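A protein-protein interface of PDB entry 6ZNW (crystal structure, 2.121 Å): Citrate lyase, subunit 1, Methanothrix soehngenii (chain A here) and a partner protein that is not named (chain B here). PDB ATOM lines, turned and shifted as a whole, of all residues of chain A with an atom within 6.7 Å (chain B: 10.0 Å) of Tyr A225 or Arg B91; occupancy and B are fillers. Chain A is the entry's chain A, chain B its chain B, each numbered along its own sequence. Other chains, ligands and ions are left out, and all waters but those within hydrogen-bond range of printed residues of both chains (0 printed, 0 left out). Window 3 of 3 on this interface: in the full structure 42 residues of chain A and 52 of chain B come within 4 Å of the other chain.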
ATOM      1  N   ASP A 221      -7.865  18.447  -3.512  1.00  0.00           N
ATOM      2  CA  ASP A 221      -9.168  17.932  -3.944  1.00  0.00           C
ATOM      3  C   ASP A 221      -9.842  16.965  -2.919  1.00  0.00           C
ATOM      4  O   ASP A 221     -11.061  16.775  -2.961  1.00  0.00           O
ATOM      5  CB  ASP A 221      -9.099  17.331  -5.364  1.00  0.00           C
ATOM      6  CG  ASP A 221      -8.499  15.948  -5.546  1.00  0.00           C
ATOM      7  OD1 ASP A 221      -7.989  15.378  -4.553  1.00  0.00           O
ATOM      8  OD2 ASP A 221      -8.522  15.442  -6.688  1.00  0.00           O
ATOM      9  N   ALA A 222      -9.065  16.425  -1.966  1.00  0.00           N
ATOM     10  CA  ALA A 222      -9.578  15.574  -0.884  1.00  0.00           C
ATOM     11  C   ALA A 222     -10.465  16.358   0.128  1.00  0.00           C
ATOM     12  O   ALA A 222     -11.190  15.744   0.916  1.00  0.00           O
ATOM     13  CB  ALA A 222      -8.417  14.919  -0.152  1.00  0.00           C
ATOM     14  N   GLU A 223     -10.391  17.704   0.103  1.00  0.00           N
ATOM     15  CA  GLU A 223     -11.147  18.619   0.963  1.00  0.00           C
ATOM     16  C   GLU A 223     -12.602  18.830   0.512  1.00  0.00           C
ATOM     17  O   GLU A 223     -13.381  19.410   1.264  1.00  0.00           O
ATOM     18  CB  GLU A 223     -10.447  19.993   1.011  1.00  0.00           C
ATOM     19  CG  GLU A 223      -9.142  19.996   1.785  1.00  0.00           C
ATOM     20  CD  GLU A 223      -9.257  20.415   3.239  1.00  0.00           C
ATOM     21  OE1 GLU A 223      -8.203  20.499   3.911  1.00  0.00           O
ATOM     22  OE2 GLU A 223     -10.392  20.670   3.705  1.00  0.00           O
ATOM     23  N   GLU A 224     -12.956  18.384  -0.709  1.00  0.00           N
ATOM     24  CA  GLU A 224     -14.267  18.546  -1.341  1.00  0.00           C
ATOM     25  C   GLU A 224     -15.481  18.366  -0.414  1.00  0.00           C
ATOM     26  O   GLU A 224     -16.375  19.208  -0.415  1.00  0.00           O
ATOM     27  CB  GLU A 224     -14.387  17.612  -2.553  1.00  0.00           C
ATOM     28  CG  GLU A 224     -15.344  18.121  -3.615  1.00  0.00           C
ATOM     29  CD  GLU A 224     -15.527  17.198  -4.805  1.00  0.00           C
ATOM     30  OE1 GLU A 224     -16.486  17.417  -5.580  1.00  0.00           O
ATOM     31  OE2 GLU A 224     -14.719  16.251  -4.958  1.00  0.00           O
ATOM     32  N   TYR A 225     -15.503  17.295   0.383  1.00  0.00           N
ATOM     33  CA  TYR A 225     -16.601  16.972   1.296  1.00  0.00           C
ATOM     34  C   TYR A 225     -16.822  18.047   2.377  1.00  0.00           C
ATOM     35  O   TYR A 225     -17.954  18.265   2.809  1.00  0.00           O
ATOM     36  CB  TYR A 225     -16.375  15.567   1.906  1.00  0.00           C
ATOM     37  CG  TYR A 225     -17.352  15.172   2.991  1.00  0.00           C
ATOM     38  CD1 TYR A 225     -18.621  14.711   2.678  1.00  0.00           C
ATOM     39  CD2 TYR A 225     -16.987  15.208   4.329  1.00  0.00           C
ATOM     40  CE1 TYR A 225     -19.523  14.350   3.670  1.00  0.00           C
ATOM     41  CE2 TYR A 225     -17.879  14.851   5.330  1.00  0.00           C
ATOM     42  CZ  TYR A 225     -19.145  14.414   4.997  1.00  0.00           C
ATOM     43  OH  TYR A 225     -20.022  14.025   5.985  1.00  0.00           O
ATOM     44  N   TRP A 226     -15.739  18.718   2.797  1.00  0.00           N
ATOM     45  CA  TRP A 226     -15.759  19.777   3.808  1.00  0.00           C
ATOM     46  C   TRP A 226     -15.848  21.189   3.215  1.00  0.00           C
ATOM     47  O   TRP A 226     -15.916  22.154   3.974  1.00  0.00           O
ATOM     48  CB  TRP A 226     -14.499  19.687   4.684  1.00  0.00           C
ATOM     49  CG  TRP A 226     -14.448  18.449   5.525  1.00  0.00           C
ATOM     50  CD1 TRP A 226     -14.964  18.286   6.776  1.00  0.00           C
ATOM     51  CD2 TRP A 226     -13.874  17.191   5.160  1.00  0.00           C
ATOM     52  NE1 TRP A 226     -14.741  17.005   7.217  1.00  0.00           N
ATOM     53  CE2 TRP A 226     -14.078  16.309   6.240  1.00  0.00           C
ATOM     54  CE3 TRP A 226     -13.195  16.725   4.028  1.00  0.00           C
ATOM     55  CZ2 TRP A 226     -13.645  14.985   6.212  1.00  0.00           C
ATOM     56  CZ3 TRP A 226     -12.804  15.406   3.990  1.00  0.00           C
ATOM     57  CH2 TRP A 226     -12.999  14.560   5.085  1.00  0.00           C
ATOM     58  N   GLN A 227     -15.799  21.325   1.879  1.00  0.00           N
ATOM     59  CA  GLN A 227     -15.817  22.627   1.222  1.00  0.00           C
ATOM     60  C   GLN A 227     -16.975  22.813   0.232  1.00  0.00           C
ATOM     61  O   GLN A 227     -16.841  23.597  -0.707  1.00  0.00           O
ATOM     62  CB  GLN A 227     -14.483  22.861   0.496  1.00  0.00           C
ATOM     63  CG  GLN A 227     -13.239  22.759   1.370  1.00  0.00           C
ATOM     64  CD  GLN A 227     -13.097  23.883   2.373  1.00  0.00           C
ATOM     65  OE1 GLN A 227     -13.666  24.981   2.231  1.00  0.00           O
ATOM     66  NE2 GLN A 227     -12.305  23.633   3.407  1.00  0.00           N
ATOM     67  N   LYS A 228     -18.113  22.139   0.447  1.00  0.00           N
ATOM     68  CA  LYS A 228     -19.269  22.233  -0.452  1.00  0.00           C
ATOM     69  C   LYS A 228     -19.823  23.656  -0.619  1.00  0.00           C
ATOM     70  O   LYS A 228     -20.347  23.987  -1.684  1.00  0.00           O
ATOM     71  CB  LYS A 228     -20.389  21.262  -0.029  1.00  0.00           C
ATOM     72  CG  LYS A 228     -19.989  19.795  -0.108  1.00  0.00           C
ATOM     73  CD  LYS A 228     -21.147  18.870   0.260  1.00  0.00           C
ATOM     74  CE  LYS A 228     -20.670  17.472   0.578  1.00  0.00           C
ATOM     75  NZ  LYS A 228     -21.795  16.508   0.695  1.00  0.00           N
ATOM     76  N   TRP A 231     -16.458  26.110  -2.219  1.00  0.00           N
ATOM     77  CA  TRP A 231     -16.102  25.710  -3.587  1.00  0.00           C
ATOM     78  C   TRP A 231     -17.303  25.635  -4.550  1.00  0.00           C
ATOM     79  O   TRP A 231     -17.127  25.203  -5.692  1.00  0.00           O
ATOM     80  CB  TRP A 231     -15.415  24.332  -3.591  1.00  0.00           C
ATOM     81  CG  TRP A 231     -14.103  24.225  -2.871  1.00  0.00           C
ATOM     82  CD1 TRP A 231     -13.510  25.157  -2.071  1.00  0.00           C
ATOM     83  CD2 TRP A 231     -13.226  23.095  -2.891  1.00  0.00           C
ATOM     84  NE1 TRP A 231     -12.319  24.673  -1.585  1.00  0.00           N
ATOM     85  CE2 TRP A 231     -12.117  23.410  -2.080  1.00  0.00           C
ATOM     86  CE3 TRP A 231     -13.258  21.855  -3.537  1.00  0.00           C
ATOM     87  CZ2 TRP A 231     -11.071  22.516  -1.877  1.00  0.00           C
ATOM     88  CZ3 TRP A 231     -12.219  20.977  -3.336  1.00  0.00           C
ATOM     89  CH2 TRP A 231     -11.140  21.312  -2.520  1.00  0.00           C
ATOM     90  N   TYR B  18     -11.687  -0.778  14.485  1.00  0.00           N
ATOM     91  CA  TYR B  18     -12.732   0.226  14.364  1.00  0.00           C
ATOM     92  C   TYR B  18     -13.399   0.012  13.001  1.00  0.00           C
ATOM     93  O   TYR B  18     -12.763   0.163  11.955  1.00  0.00           O
ATOM     94  CB  TYR B  18     -12.177   1.665  14.487  1.00  0.00           C
ATOM     95  CG  TYR B  18     -13.282   2.697  14.525  1.00  0.00           C
ATOM     96  CD1 TYR B  18     -13.911   3.111  13.363  1.00  0.00           C
ATOM     97  CD2 TYR B  18     -13.758   3.186  15.730  1.00  0.00           C
ATOM     98  CE1 TYR B  18     -14.962   4.019  13.393  1.00  0.00           C
ATOM     99  CE2 TYR B  18     -14.809   4.097  15.776  1.00  0.00           C
ATOM    100  CZ  TYR B  18     -15.420   4.500  14.603  1.00  0.00           C
ATOM    101  OH  TYR B  18     -16.452   5.415  14.619  1.00  0.00           O
ATOM    102  N   ASN B  86      -8.056   1.234  12.155  1.00  0.00           N
ATOM    103  CA  ASN B  86      -9.141   2.137  11.802  1.00  0.00           C
ATOM    104  C   ASN B  86      -9.641   1.985  10.364  1.00  0.00           C
ATOM    105  O   ASN B  86      -8.988   2.418   9.413  1.00  0.00           O
ATOM    106  CB  ASN B  86      -8.703   3.587  12.091  1.00  0.00           C
ATOM    107  CG  ASN B  86      -9.805   4.607  12.094  1.00  0.00           C
ATOM    108  OD1 ASN B  86     -10.961   4.303  11.835  1.00  0.00           O
ATOM    109  ND2 ASN B  86      -9.468   5.846  12.392  1.00  0.00           N
ATOM    110  N   PHE B  87     -10.829   1.401  10.218  1.00  0.00           N
ATOM    111  CA  PHE B  87     -11.472   1.234   8.917  1.00  0.00           C
ATOM    112  C   PHE B  87     -12.530   2.303   8.654  1.00  0.00           C
ATOM    113  O   PHE B  87     -13.339   2.126   7.746  1.00  0.00           O
ATOM    114  CB  PHE B  87     -12.090  -0.172   8.763  1.00  0.00           C
ATOM    115  CG  PHE B  87     -11.080  -1.276   8.554  1.00  0.00           C
ATOM    116  CD1 PHE B  87     -10.474  -1.459   7.322  1.00  0.00           C
ATOM    117  CD2 PHE B  87     -10.751  -2.143   9.582  1.00  0.00           C
ATOM    118  CE1 PHE B  87      -9.527  -2.454   7.134  1.00  0.00           C
ATOM    119  CE2 PHE B  87      -9.830  -3.166   9.380  1.00  0.00           C
ATOM    120  CZ  PHE B  87      -9.205  -3.298   8.162  1.00  0.00           C
ATOM    121  N   ALA B  88     -12.528   3.424   9.408  1.00  0.00           N
ATOM    122  CA  ALA B  88     -13.486   4.502   9.160  1.00  0.00           C
ATOM    123  C   ALA B  88     -13.254   5.095   7.766  1.00  0.00           C
ATOM    124  O   ALA B  88     -12.129   5.066   7.262  1.00  0.00           O
ATOM    125  CB  ALA B  88     -13.352   5.596  10.211  1.00  0.00           C
ATOM    126  N   SER B  89     -14.328   5.593   7.137  1.00  0.00           N
ATOM    127  CA  SER B  89     -14.264   6.233   5.825  1.00  0.00           C
ATOM    128  C   SER B  89     -13.403   7.515   5.899  1.00  0.00           C
ATOM    129  O   SER B  89     -13.099   7.979   7.000  1.00  0.00           O
ATOM    130  CB  SER B  89     -15.676   6.592   5.360  1.00  0.00           C
ATOM    131  OG  SER B  89     -16.206   7.734   6.022  1.00  0.00           O
ATOM    132  N   HIS B  90     -13.040   8.108   4.741  1.00  0.00           N
ATOM    133  CA  HIS B  90     -12.267   9.357   4.747  1.00  0.00           C
ATOM    134  C   HIS B  90     -13.037  10.511   5.425  1.00  0.00           C
ATOM    135  O   HIS B  90     -12.418  11.483   5.870  1.00  0.00           O
ATOM    136  CB  HIS B  90     -11.796   9.742   3.333  1.00  0.00           C
ATOM    137  CG  HIS B  90     -12.885  10.211   2.419  1.00  0.00           C
ATOM    138  ND1 HIS B  90     -13.668   9.317   1.710  1.00  0.00           N
ATOM    139  CD2 HIS B  90     -13.266  11.471   2.101  1.00  0.00           C
ATOM    140  CE1 HIS B  90     -14.508  10.058   1.001  1.00  0.00           C
ATOM    141  NE2 HIS B  90     -14.310  11.359   1.208  1.00  0.00           N
ATOM    142  N   ARG B  91     -14.377  10.387   5.534  1.00  0.00           N
ATOM    143  CA  ARG B  91     -15.239  11.369   6.172  1.00  0.00           C
ATOM    144  C   ARG B  91     -15.129  11.358   7.686  1.00  0.00           C
ATOM    145  O   ARG B  91     -15.395  12.392   8.308  1.00  0.00           O
ATOM    146  CB  ARG B  91     -16.695  11.185   5.733  1.00  0.00           C
ATOM    147  CG  ARG B  91     -16.898  11.408   4.229  1.00  0.00           C
ATOM    148  CD  ARG B  91     -18.284  11.006   3.736  1.00  0.00           C
ATOM    149  NE  ARG B  91     -18.640   9.645   4.144  1.00  0.00           N
ATOM    150  CZ  ARG B  91     -18.441   8.557   3.408  1.00  0.00           C
ATOM    151  NH1 ARG B  91     -18.772   7.362   3.878  1.00  0.00           N
ATOM    152  NH2 ARG B  91     -17.919   8.656   2.191  1.00  0.00           N
ATOM    153  N   SER B  92     -14.708  10.234   8.286  1.00  0.00           N
ATOM    154  CA  SER B  92     -14.581  10.164   9.734  1.00  0.00           C
ATOM    155  C   SER B  92     -13.221   9.677  10.234  1.00  0.00           C
ATOM    156  O   SER B  92     -13.043   9.590  11.441  1.00  0.00           O
ATOM    157  CB  SER B  92     -15.703   9.323  10.331  1.00  0.00           C
ATOM    158  OG  SER B  92     -15.811   8.059   9.701  1.00  0.00           O
ATOM    159  N   ALA B  93     -12.265   9.379   9.333  1.00  0.00           N
ATOM    160  CA  ALA B  93     -10.931   8.887   9.694  1.00  0.00           C
ATOM    161  C   ALA B  93     -10.178   9.816  10.643  1.00  0.00           C
ATOM    162  O   ALA B  93      -9.556   9.328  11.584  1.00  0.00           O
ATOM    163  CB  ALA B  93     -10.098   8.635   8.450  1.00  0.00           C
ATOM    164  N   PHE B  94     -10.250  11.145  10.423  1.00  0.00           N
ATOM    165  CA  PHE B  94      -9.562  12.110  11.283  1.00  0.00           C
ATOM    166  C   PHE B  94     -10.105  12.130  12.704  1.00  0.00           C
ATOM    167  O   PHE B  94      -9.326  11.940  13.628  1.00  0.00           O
ATOM    168  CB  PHE B  94      -9.579  13.526  10.681  1.00  0.00           C
ATOM    169  CG  PHE B  94      -8.957  14.612  11.533  1.00  0.00           C
ATOM    170  CD1 PHE B  94      -7.588  14.788  11.565  1.00  0.00           C
ATOM    171  CD2 PHE B  94      -9.748  15.489  12.256  1.00  0.00           C
ATOM    172  CE1 PHE B  94      -7.017  15.806  12.320  1.00  0.00           C
ATOM    173  CE2 PHE B  94      -9.176  16.507  13.012  1.00  0.00           C
ATOM    174  CZ  PHE B  94      -7.814  16.663  13.032  1.00  0.00           C
ATOM    175  N   GLU B  95     -11.418  12.370  12.889  1.00  0.00           N
ATOM    176  CA  GLU B  95     -11.983  12.451  14.232  1.00  0.00           C
ATOM    177  C   GLU B  95     -11.852  11.144  15.023  1.00  0.00           C
ATOM    178  O   GLU B  95     -11.583  11.206  16.219  1.00  0.00           O
ATOM    179  CB  GLU B  95     -13.424  12.985  14.234  1.00  0.00           C
ATOM    180  CG  GLU B  95     -14.475  12.100  13.592  1.00  0.00           C
ATOM    181  CD  GLU B  95     -15.688  12.908  13.177  1.00  0.00           C
ATOM    182  OE1 GLU B  95     -16.591  13.108  14.022  1.00  0.00           O
ATOM    183  OE2 GLU B  95     -15.715  13.375  12.015  1.00  0.00           O
ATOM    184  N   THR B  96     -11.957   9.978  14.366  1.00  0.00           N
ATOM    185  CA  THR B  96     -11.805   8.694  15.048  1.00  0.00           C
ATOM    186  C   THR B  96     -10.335   8.429  15.423  1.00  0.00           C
ATOM    187  O   THR B  96     -10.076   7.932  16.516  1.00  0.00           O
ATOM    188  CB  THR B  96     -12.455   7.558  14.247  1.00  0.00           C
ATOM    189  OG1 THR B  96     -11.846   7.484  12.962  1.00  0.00           O
ATOM    190  CG2 THR B  96     -13.955   7.736  14.103  1.00  0.00           C
ATOM    191  N   THR B  97      -9.375   8.796  14.552  1.00  0.00           N
ATOM    192  CA  THR B  97      -7.950   8.628  14.861  1.00  0.00           C
ATOM    193  C   THR B  97      -7.551   9.570  15.992  1.00  0.00           C
ATOM    194  O   THR B  97      -6.846   9.159  16.909  1.00  0.00           O
ATOM    195  CB  THR B  97      -7.077   8.873  13.626  1.00  0.00           C
ATOM    196  OG1 THR B  97      -7.476   7.988  12.579  1.00  0.00           O
ATOM    197  CG2 THR B  97      -5.587   8.715  13.916  1.00  0.00           C
ATOM    198  N   VAL B 111      -4.483   3.997   9.829  1.00  0.00           N
ATOM    199  CA  VAL B 111      -5.563   4.639   9.082  1.00  0.00           C
ATOM    200  C   VAL B 111      -5.608   4.082   7.669  1.00  0.00           C
ATOM    201  O   VAL B 111      -4.687   4.317   6.889  1.00  0.00           O
ATOM    202  CB  VAL B 111      -5.421   6.173   9.077  1.00  0.00           C
ATOM    203  CG1 VAL B 111      -6.648   6.827   8.439  1.00  0.00           C
ATOM    204  CG2 VAL B 111      -5.187   6.706  10.485  1.00  0.00           C
ATOM    205  N   ILE B 112      -6.670   3.345   7.343  1.00  0.00           N
ATOM    206  CA  ILE B 112      -6.812   2.678   6.054  1.00  0.00           C
ATOM    207  C   ILE B 112      -7.359   3.622   4.952  1.00  0.00           C
ATOM    208  O   ILE B 112      -6.944   3.527   3.789  1.00  0.00           O
ATOM    209  CB  ILE B 112      -7.686   1.368   6.242  1.00  0.00           C
ATOM    210  CG1 ILE B 112      -6.872   0.193   6.857  1.00  0.00           C
ATOM    211  CG2 ILE B 112      -8.318   0.900   4.942  1.00  0.00           C
ATOM    212  CD1 ILE B 112      -6.172   0.403   8.161  1.00  0.00           C
ATOM    213  N   ALA B 113      -8.284   4.524   5.325  1.00  0.00           N
ATOM    214  CA  ALA B 113      -8.989   5.407   4.404  1.00  0.00           C
ATOM    215  C   ALA B 113      -8.130   6.167   3.393  1.00  0.00           C
ATOM    216  O   ALA B 113      -7.083   6.718   3.723  1.00  0.00           O
ATOM    217  CB  ALA B 113      -9.850   6.393   5.171  1.00  0.00           C
ATOM    218  N   GLU B 114      -8.605   6.178   2.151  1.00  0.00           N
ATOM    219  CA  GLU B 114      -8.045   6.924   1.034  1.00  0.00           C
ATOM    220  C   GLU B 114      -8.930   8.169   0.881  1.00  0.00           C
ATOM    221  O   GLU B 114     -10.154   8.090   1.052  1.00  0.00           O
ATOM    222  CB  GLU B 114      -8.137   6.110  -0.268  1.00  0.00           C
ATOM    223  CG  GLU B 114      -7.565   4.710  -0.164  1.00  0.00           C
ATOM    224  CD  GLU B 114      -6.148   4.563  -0.678  1.00  0.00           C
ATOM    225  OE1 GLU B 114      -5.686   5.463  -1.425  1.00  0.00           O
ATOM    226  OE2 GLU B 114      -5.495   3.550  -0.330  1.00  0.00           O
ATOM    227  N   GLY B 115      -8.317   9.295   0.549  1.00  0.00           N
ATOM    228  CA  GLY B 115      -9.048  10.541   0.347  1.00  0.00           C
ATOM    229  C   GLY B 115      -9.137  11.432   1.567  1.00  0.00           C
ATOM    230  O   GLY B 115     -10.036  12.272   1.655  1.00  0.00           O
ATOM    231  N   VAL B 116      -8.203  11.264   2.518  1.00  0.00           N
ATOM    232  CA  VAL B 116      -8.145  12.087   3.720  1.00  0.00           C
ATOM    233  C   VAL B 116      -7.397  13.395   3.390  1.00  0.00           C
ATOM    234  O   VAL B 116      -6.302  13.350   2.818  1.00  0.00           O
ATOM    235  CB  VAL B 116      -7.458  11.320   4.880  1.00  0.00           C
ATOM    236  CG1 VAL B 116      -7.275  12.212   6.107  1.00  0.00           C
ATOM    237  CG2 VAL B 116      -8.229  10.045   5.238  1.00  0.00           C
ATOM    238  N   PRO B 117      -7.971  14.577   3.724  1.00  0.00           N
ATOM    239  CA  PRO B 117      -7.280  15.845   3.435  1.00  0.00           C
ATOM    240  C   PRO B 117      -5.846  15.906   3.947  1.00  0.00           C
ATOM    241  O   PRO B 117      -5.529  15.315   4.984  1.00  0.00           O
ATOM    242  CB  PRO B 117      -8.148  16.892   4.143  1.00  0.00           C
ATOM    243  CG  PRO B 117      -9.482  16.297   4.203  1.00  0.00           C
ATOM    244  CD  PRO B 117      -9.272  14.817   4.374  1.00  0.00           C
ATOM    245  N   GLN B 120      -5.570  17.411   7.507  1.00  0.00           N
ATOM    246  CA  GLN B 120      -5.962  16.463   8.552  1.00  0.00           C
ATOM    247  C   GLN B 120      -4.813  15.500   8.862  1.00  0.00           C
ATOM    248  O   GLN B 120      -4.506  15.281  10.028  1.00  0.00           O
ATOM    249  CB  GLN B 120      -7.216  15.695   8.120  1.00  0.00           C
ATOM    250  CG  GLN B 120      -8.493  16.516   8.231  1.00  0.00           C
ATOM    251  CD  GLN B 120      -9.716  15.760   7.779  1.00  0.00           C
ATOM    252  OE1 GLN B 120      -9.736  14.527   7.703  1.00  0.00           O
ATOM    253  NE2 GLN B 120     -10.772  16.486   7.461  1.00  0.00           N
ATOM    254  N   PRO B 138      -2.558   7.893   6.418  1.00  0.00           N
ATOM    255  CA  PRO B 138      -3.717   7.243   5.773  1.00  0.00           C
ATOM    256  C   PRO B 138      -3.370   6.549   4.441  1.00  0.00           C
ATOM    257  O   PRO B 138      -2.214   6.544   4.010  1.00  0.00           O
ATOM    258  CB  PRO B 138      -4.728   8.404   5.606  1.00  0.00           C
ATOM    259  CG  PRO B 138      -4.164   9.578   6.370  1.00  0.00           C
ATOM    260  CD  PRO B 138      -2.681   9.364   6.369  1.00  0.00           C
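Gly B115 touches Ala A222 (O to CB, 3.6 Å).
Val B116 touches Ala A222 (O to CB, 3.97 Å).
Pro B117 touches Ala A222.
Glu A223 touches Pro B117.
Tyr A225 touches Arg B91.
CH2 of Trp A226 touches O of His B90, at 3.2 Å.
Arg B91 touches Trp A226.
Trp A226 touches Pro B117.
Gln B120 touches Trp A226 (NE2 to CZ2, 3.5 Å).
Printed residues of chain B within 4 Å of Ala A222: Gly B115 (3.6 Å), Val B116 (3.97 Å) and Pro B117 (3.7 Å).
Printed residues of chain B within 4 Å of Glu A223: Pro B117 (3.6 Å).
Of chain B, only Arg B91 (3.6 Å) comes within 4 Å of Tyr A225.
Of the printed residues of chain B, Trp A226 touches His B90, Arg B91, Pro B117 and Gln B120.
Printed residues of chain A within 4 Å of His B90: Trp A226.
Arg B91 touches just these residues of chain A: Tyr A225 (3.6 Å) and Trp A226 (3.8 Å).
Thr B97 touches none of the printed residues of chain A.
Printed residues of chain A within 4 Å of Gly B115: Ala A222.
Printed residues of chain A within 4 Å of Pro B117: Ala A222, Glu A223 and Trp A226.
The nearest printed residue of chain A that does not touch Arg B91 is Lys A228 (7.2 Å).
Hydrophobic or aromatic side chains of chain B within 4 Å of the printed part of chain A: Pro B117.
Of the 9 printed residues of chain A, 4 touch a printed residue of chain B.
Printed residues of chain A that touch a printed residue of chain B: Ala A222, Glu A223, Tyr A225 and Trp A226.
Hydrophobic or aromatic side chains of chain A within 4 Å of the printed part of chain B: Ala A222, Tyr A225 and Trp A226.
Among the printed residues, no Asp or Glu carboxylate lies within 4 Å of a Lys or Arg side-chain nitrogen of the other chain.
The backbone NH of Arg B91 lies close to the side-chain hydroxyl of Ser B89, at 3.3 Å.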
